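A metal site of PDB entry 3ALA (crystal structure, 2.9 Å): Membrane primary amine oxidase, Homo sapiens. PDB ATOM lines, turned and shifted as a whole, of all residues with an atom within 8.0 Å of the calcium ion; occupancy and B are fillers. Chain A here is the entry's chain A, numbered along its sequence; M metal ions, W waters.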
ATOM      1  N   LYS A  91      -3.316  17.867  17.583  1.00  0.00           N
ATOM      2  CA  LYS A  91      -4.013  17.677  18.854  1.00  0.00           C
ATOM      3  C   LYS A  91      -5.323  16.918  18.662  1.00  0.00           C
ATOM      4  O   LYS A  91      -5.594  15.974  19.367  1.00  0.00           O
ATOM      5  CB  LYS A  91      -4.294  19.021  19.580  1.00  0.00           C
ATOM      6  CG  LYS A  91      -4.220  18.904  21.087  1.00  0.00           C
ATOM      7  CD  LYS A  91      -5.209  19.755  21.875  1.00  0.00           C
ATOM      8  CE  LYS A  91      -4.664  21.106  22.178  1.00  0.00           C
ATOM      9  NZ  LYS A  91      -5.240  21.752  23.370  1.00  0.00           N
ATOM     10  N   LEU A 344      -5.237  17.729  33.001  1.00  0.00           N
ATOM     11  CA  LEU A 344      -5.102  19.146  33.318  1.00  0.00           C
ATOM     12  C   LEU A 344      -4.431  19.864  32.183  1.00  0.00           C
ATOM     13  O   LEU A 344      -4.848  20.935  31.759  1.00  0.00           O
ATOM     14  CB  LEU A 344      -4.269  19.350  34.599  1.00  0.00           C
ATOM     15  CG  LEU A 344      -4.820  18.718  35.878  1.00  0.00           C
ATOM     16  CD1 LEU A 344      -3.843  18.860  37.046  1.00  0.00           C
ATOM     17  CD2 LEU A 344      -6.171  19.327  36.216  1.00  0.00           C
ATOM     18  N   VAL A 345      -3.348  19.272  31.698  1.00  0.00           N
ATOM     19  CA  VAL A 345      -2.571  19.901  30.645  1.00  0.00           C
ATOM     20  C   VAL A 345      -2.369  18.934  29.499  1.00  0.00           C
ATOM     21  O   VAL A 345      -2.096  17.791  29.727  1.00  0.00           O
ATOM     22  CB  VAL A 345      -1.187  20.345  31.153  1.00  0.00           C
ATOM     23  CG1 VAL A 345      -0.454  21.024  30.184  1.00  0.00           C
ATOM     24  CG2 VAL A 345      -1.124  20.719  32.576  1.00  0.00           C
ATOM     25  N   TYR A 346      -2.541  19.418  28.275  1.00  0.00           N
ATOM     26  CA  TYR A 346      -2.163  18.665  27.098  1.00  0.00           C
ATOM     27  C   TYR A 346      -0.643  18.712  26.935  1.00  0.00           C
ATOM     28  O   TYR A 346      -0.018  17.703  26.652  1.00  0.00           O
ATOM     29  CB  TYR A 346      -2.850  19.227  25.833  1.00  0.00           C
ATOM     30  CG  TYR A 346      -2.445  18.534  24.547  1.00  0.00           C
ATOM     31  CD1 TYR A 346      -2.992  17.316  24.173  1.00  0.00           C
ATOM     32  CD2 TYR A 346      -1.491  19.086  23.701  1.00  0.00           C
ATOM     33  CE1 TYR A 346      -2.611  16.674  23.015  1.00  0.00           C
ATOM     34  CE2 TYR A 346      -1.108  18.446  22.534  1.00  0.00           C
ATOM     35  CZ  TYR A 346      -1.669  17.228  22.189  1.00  0.00           C
ATOM     36  OH  TYR A 346      -1.305  16.574  21.026  1.00  0.00           O
ATOM     37  N   GLU A 347      -0.048  19.893  27.115  1.00  0.00           N
ATOM     38  CA  GLU A 347       1.367  20.035  26.892  1.00  0.00           C
ATOM     39  C   GLU A 347       1.939  21.116  27.769  1.00  0.00           C
ATOM     40  O   GLU A 347       1.378  22.157  27.831  1.00  0.00           O
ATOM     41  CB  GLU A 347       1.616  20.410  25.424  1.00  0.00           C
ATOM     42  CG  GLU A 347       3.067  20.793  25.082  1.00  0.00           C
ATOM     43  CD  GLU A 347       3.228  21.473  23.703  1.00  0.00           C
ATOM     44  OE1 GLU A 347       2.251  21.575  22.914  1.00  0.00           O
ATOM     45  OE2 GLU A 347       4.353  21.952  23.402  1.00  0.00           O
ATOM     46  N   VAL A 513       2.398  26.583  27.814  1.00  0.00           N
ATOM     47  CA  VAL A 513       1.564  25.927  28.772  1.00  0.00           C
ATOM     48  C   VAL A 513       0.183  25.788  28.151  1.00  0.00           C
ATOM     49  O   VAL A 513      -0.576  26.751  28.110  1.00  0.00           O
ATOM     50  CB  VAL A 513       1.479  26.747  30.074  1.00  0.00           C
ATOM     51  CG1 VAL A 513       0.741  25.986  31.152  1.00  0.00           C
ATOM     52  CG2 VAL A 513       2.844  27.114  30.557  1.00  0.00           C
ATOM     53  N   ASP A 514      -0.130  24.609  27.623  1.00  0.00           N
ATOM     54  CA  ASP A 514      -1.414  24.356  27.017  1.00  0.00           C
ATOM     55  C   ASP A 514      -2.295  23.573  27.978  1.00  0.00           C
ATOM     56  O   ASP A 514      -2.459  22.352  27.874  1.00  0.00           O
ATOM     57  CB  ASP A 514      -1.285  23.595  25.711  1.00  0.00           C
ATOM     58  CG  ASP A 514      -2.627  23.316  25.052  1.00  0.00           C
ATOM     59  OD1 ASP A 514      -3.668  23.871  25.455  1.00  0.00           O
ATOM     60  OD2 ASP A 514      -2.629  22.498  24.126  1.00  0.00           O
ATOM     61  N   LEU A 515      -2.873  24.334  28.892  1.00  0.00           N
ATOM     62  CA  LEU A 515      -3.875  23.847  29.814  1.00  0.00           C
ATOM     63  C   LEU A 515      -5.127  23.576  29.066  1.00  0.00           C
ATOM     64  O   LEU A 515      -5.480  24.326  28.198  1.00  0.00           O
ATOM     65  CB  LEU A 515      -4.178  24.930  30.852  1.00  0.00           C
ATOM     66  CG  LEU A 515      -3.247  24.993  32.061  1.00  0.00           C
ATOM     67  CD1 LEU A 515      -3.215  26.383  32.533  1.00  0.00           C
ATOM     68  CD2 LEU A 515      -3.687  24.008  33.165  1.00  0.00           C
ATOM     69  N   ASP A 516      -5.800  22.488  29.392  1.00  0.00           N
ATOM     70  CA  ASP A 516      -7.136  22.253  28.874  1.00  0.00           C
ATOM     71  C   ASP A 516      -8.034  22.020  30.047  1.00  0.00           C
ATOM     72  O   ASP A 516      -8.345  20.883  30.346  1.00  0.00           O
ATOM     73  CB  ASP A 516      -7.160  21.005  27.997  1.00  0.00           C
ATOM     74  CG  ASP A 516      -6.515  21.199  26.638  1.00  0.00           C
ATOM     75  OD1 ASP A 516      -6.195  22.340  26.208  1.00  0.00           O
ATOM     76  OD2 ASP A 516      -6.352  20.145  25.984  1.00  0.00           O
ATOM     77  N   VAL A 517      -8.459  23.097  30.709  1.00  0.00           N
ATOM     78  CA  VAL A 517      -9.129  22.979  32.005  1.00  0.00           C
ATOM     79  C   VAL A 517     -10.525  22.399  31.841  1.00  0.00           C
ATOM     80  O   VAL A 517     -11.395  23.027  31.278  1.00  0.00           O
ATOM     81  CB  VAL A 517      -9.210  24.336  32.762  1.00  0.00           C
ATOM     82  CG1 VAL A 517      -9.521  24.097  34.234  1.00  0.00           C
ATOM     83  CG2 VAL A 517      -7.910  25.126  32.610  1.00  0.00           C
ATOM     84  N   GLY A 519     -11.731  20.165  29.851  1.00  0.00           N
ATOM     85  CA  GLY A 519     -12.085  20.238  28.430  1.00  0.00           C
ATOM     86  C   GLY A 519     -11.256  21.256  27.665  1.00  0.00           C
ATOM     87  O   GLY A 519     -10.392  21.904  28.245  1.00  0.00           O
ATOM     88  N   LEU A 520     -11.516  21.409  26.373  1.00  0.00           N
ATOM     89  CA  LEU A 520     -10.739  22.368  25.538  1.00  0.00           C
ATOM     90  C   LEU A 520     -11.132  23.809  25.732  1.00  0.00           C
ATOM     91  O   LEU A 520     -10.285  24.659  25.904  1.00  0.00           O
ATOM     92  CB  LEU A 520     -10.889  22.057  24.052  1.00  0.00           C
ATOM     93  CG  LEU A 520     -10.203  20.837  23.446  1.00  0.00           C
ATOM     94  CD1 LEU A 520     -10.353  20.982  21.943  1.00  0.00           C
ATOM     95  CD2 LEU A 520      -8.751  20.712  23.849  1.00  0.00           C
ATOM     96  N   GLU A 521     -12.425  24.069  25.661  1.00  0.00           N
ATOM     97  CA  GLU A 521     -12.957  25.430  25.678  1.00  0.00           C
ATOM     98  C   GLU A 521     -12.706  26.117  27.027  1.00  0.00           C
ATOM     99  O   GLU A 521     -13.218  25.700  28.051  1.00  0.00           O
ATOM    100  CB  GLU A 521     -14.463  25.428  25.389  1.00  0.00           C
ATOM    101  CG  GLU A 521     -14.838  24.986  23.982  1.00  0.00           C
ATOM    102  CD  GLU A 521     -14.858  23.420  23.831  1.00  0.00           C
ATOM    103  OE1 GLU A 521     -14.808  22.697  24.875  1.00  0.00           O
ATOM    104  OE2 GLU A 521     -14.899  22.884  22.691  1.00  0.00           O
ATOM    105  N   ASN A 522     -11.919  27.172  27.009  1.00  0.00           N
ATOM    106  CA  ASN A 522     -11.557  27.820  28.223  1.00  0.00           C
ATOM    107  C   ASN A 522     -11.686  29.338  28.089  1.00  0.00           C
ATOM    108  O   ASN A 522     -11.737  29.850  27.010  1.00  0.00           O
ATOM    109  CB  ASN A 522     -10.122  27.454  28.604  1.00  0.00           C
ATOM    110  CG  ASN A 522      -9.994  26.038  29.175  1.00  0.00           C
ATOM    111  OD1 ASN A 522      -8.897  25.532  29.310  1.00  0.00           O
ATOM    112  ND2 ASN A 522     -11.100  25.432  29.530  1.00  0.00           N
ATOM    113  N   LEU A 574      -7.182  30.367  34.080  1.00  0.00           N
ATOM    114  CA  LEU A 574      -7.915  29.881  32.931  1.00  0.00           C
ATOM    115  C   LEU A 574      -8.976  28.956  33.443  1.00  0.00           C
ATOM    116  O   LEU A 574      -8.683  28.162  34.336  1.00  0.00           O
ATOM    117  CB  LEU A 574      -6.999  29.131  31.985  1.00  0.00           C
ATOM    118  CG  LEU A 574      -6.282  29.983  30.961  1.00  0.00           C
ATOM    119  CD1 LEU A 574      -5.317  30.946  31.598  1.00  0.00           C
ATOM    120  CD2 LEU A 574      -5.549  29.084  29.985  1.00  0.00           C
ATOM    121  N   THR A 620      -3.079  33.041  24.170  1.00  0.00           N
ATOM    122  CA  THR A 620      -3.502  33.117  22.790  1.00  0.00           C
ATOM    123  C   THR A 620      -4.315  31.894  22.408  1.00  0.00           C
ATOM    124  O   THR A 620      -4.276  30.886  23.075  1.00  0.00           O
ATOM    125  CB  THR A 620      -2.319  33.167  21.884  1.00  0.00           C
ATOM    126  OG1 THR A 620      -1.578  31.974  22.047  1.00  0.00           O
ATOM    127  CG2 THR A 620      -1.458  34.307  22.218  1.00  0.00           C
ATOM    128  N   GLN A 621      -5.057  32.000  21.326  1.00  0.00           N
ATOM    129  CA  GLN A 621      -5.747  30.841  20.788  1.00  0.00           C
ATOM    130  C   GLN A 621      -4.686  29.830  20.454  1.00  0.00           C
ATOM    131  O   GLN A 621      -3.660  30.211  19.918  1.00  0.00           O
ATOM    132  CB  GLN A 621      -6.506  31.188  19.518  1.00  0.00           C
ATOM    133  CG  GLN A 621      -7.810  31.914  19.748  1.00  0.00           C
ATOM    134  CD  GLN A 621      -8.638  32.119  18.496  1.00  0.00           C
ATOM    135  OE1 GLN A 621      -8.679  31.254  17.608  1.00  0.00           O
ATOM    136  NE2 GLN A 621      -9.291  33.269  18.409  1.00  0.00           N
ATOM    137  N   ARG A 622      -4.895  28.570  20.798  1.00  0.00           N
ATOM    138  CA  ARG A 622      -3.987  27.519  20.344  1.00  0.00           C
ATOM    139  C   ARG A 622      -4.271  27.177  18.895  1.00  0.00           C
ATOM    140  O   ARG A 622      -5.435  27.060  18.513  1.00  0.00           O
ATOM    141  CB  ARG A 622      -4.129  26.258  21.158  1.00  0.00           C
ATOM    142  CG  ARG A 622      -3.031  25.277  20.856  1.00  0.00           C
ATOM    143  CD  ARG A 622      -3.468  23.880  21.072  1.00  0.00           C
ATOM    144  NE  ARG A 622      -2.455  22.882  20.693  1.00  0.00           N
ATOM    145  CZ  ARG A 622      -2.214  22.497  19.455  1.00  0.00           C
ATOM    146  NH1 ARG A 622      -2.871  23.032  18.426  1.00  0.00           N
ATOM    147  NH2 ARG A 622      -1.304  21.575  19.228  1.00  0.00           N
ATOM    148  N   LYS A 657     -12.201  29.318  23.742  1.00  0.00           N
ATOM    149  CA  LYS A 657     -11.465  28.569  22.760  1.00  0.00           C
ATOM    150  C   LYS A 657     -10.475  27.629  23.432  1.00  0.00           C
ATOM    151  O   LYS A 657     -10.333  27.629  24.641  1.00  0.00           O
ATOM    152  CB  LYS A 657     -10.703  29.516  21.861  1.00  0.00           C
ATOM    153  CG  LYS A 657     -11.532  30.659  21.338  1.00  0.00           C
ATOM    154  CD  LYS A 657     -12.658  30.165  20.418  1.00  0.00           C
ATOM    155  CE  LYS A 657     -12.471  30.639  18.967  1.00  0.00           C
ATOM    156  NZ  LYS A 657     -13.760  30.529  18.210  1.00  0.00           N
ATOM    157  N   ASP A 658      -9.819  26.795  22.640  1.00  0.00           N
ATOM    158  CA  ASP A 658      -8.636  26.082  23.101  1.00  0.00           C
ATOM    159  C   ASP A 658      -7.537  27.098  23.275  1.00  0.00           C
ATOM    160  O   ASP A 658      -7.053  27.656  22.301  1.00  0.00           O
ATOM    161  CB  ASP A 658      -8.216  25.028  22.116  1.00  0.00           C
ATOM    162  CG  ASP A 658      -7.048  24.226  22.591  1.00  0.00           C
ATOM    163  OD1 ASP A 658      -6.366  24.699  23.484  1.00  0.00           O
ATOM    164  OD2 ASP A 658      -6.841  23.119  22.057  1.00  0.00           O
ATOM    165  N   LEU A 659      -7.170  27.364  24.519  1.00  0.00           N
ATOM    166  CA  LEU A 659      -6.247  28.427  24.839  1.00  0.00           C
ATOM    167  C   LEU A 659      -4.917  27.828  25.218  1.00  0.00           C
ATOM    168  O   LEU A 659      -4.818  26.649  25.547  1.00  0.00           O
ATOM    169  CB  LEU A 659      -6.759  29.268  25.991  1.00  0.00           C
ATOM    170  CG  LEU A 659      -8.055  30.049  25.791  1.00  0.00           C
ATOM    171  CD1 LEU A 659      -8.456  30.650  27.114  1.00  0.00           C
ATOM    172  CD2 LEU A 659      -7.899  31.126  24.744  1.00  0.00           C
ATOM    173  N   VAL A 660      -3.898  28.677  25.158  1.00  0.00           N
ATOM    174  CA  VAL A 660      -2.531  28.309  25.508  1.00  0.00           C
ATOM    175  C   VAL A 660      -1.796  29.492  26.087  1.00  0.00           C
ATOM    176  O   VAL A 660      -1.743  30.545  25.461  1.00  0.00           O
ATOM    177  CB  VAL A 660      -1.744  27.776  24.294  1.00  0.00           C
ATOM    178  CG1 VAL A 660      -1.784  28.737  23.158  1.00  0.00           C
ATOM    179  CG2 VAL A 660      -0.323  27.527  24.661  1.00  0.00           C
ATOM    180  N   ALA A 661      -1.231  29.302  27.284  1.00  0.00           N
ATOM    181  CA  ALA A 661      -0.510  30.365  27.954  1.00  0.00           C
ATOM    182  C   ALA A 661       0.944  30.277  27.636  1.00  0.00           C
ATOM    183  O   ALA A 661       1.472  29.204  27.442  1.00  0.00           O
ATOM    184  CB  ALA A 661      -0.695  30.271  29.417  1.00  0.00           C
HETATM  185 CA    CA M   1      -5.737  24.458  25.747  1.00  0.00          CA
HETATM  186  O   HOH W   1      -7.860  25.441  26.209  1.00  0.00           O
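O of Asp 514 is in hydrogen-bond range of N of Tyr 346 (3.0 Å). The side-chain carboxylate (OD2) of Asp 516 lies within salt-bridge range of the side-chain amino group (NZ) of Lys 91, 3.3 Å away. The backbone carbonyl oxygen (O) of Asp 658 is in hydrogen-bond range of the backbone NH (N) of Arg 622 (2.8 Å). N of Asp 514 lies within hydrogen-bond range of O of Glu 347 (2.9 Å). The backbone NH (N) of Asp 516 sits at hydrogen-bond distance from the backbone carbonyl oxygen (O) of Leu 344, at 3.0 Å. OD2 of Asp 658 is in salt-bridge range of NZ of Lys 91, at 2.5 Å. OD2 of Asp 514 is in salt-bridge range of NZ of Lys 91 (2.8 Å). The side-chain carboxylate (OD2) of Asp 514 lies within salt-bridge range of the guanidinium group (NE) of Arg 622 (3.5 Å).
Lys 91 touches the calcium ion (NZ to CA, 3.6 Å). Within 4 Å of the calcium ion: Lys 91, Asp 514, Leu 515, Asp 516, Asp 658 and Leu 659. The nearest printed residue that does not touch the calcium ion is Leu 520 (4.6 Å).
The calcium ion is bound by OD1 of Asp 514 (2.2 Å), OD1 of Asp 516 (2.2 Å), OD1 of Asp 658 (2.4 Å), O of Leu 659 (2.4 Å), water W1 (2.4 Å) and O of Leu 515 (2.5 Å). The calcium ion has six donor atoms within binding distance.
Water W1 lies within hydrogen-bond range of O of Leu 520, N of Leu 659 and OD1 of Asn 522.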
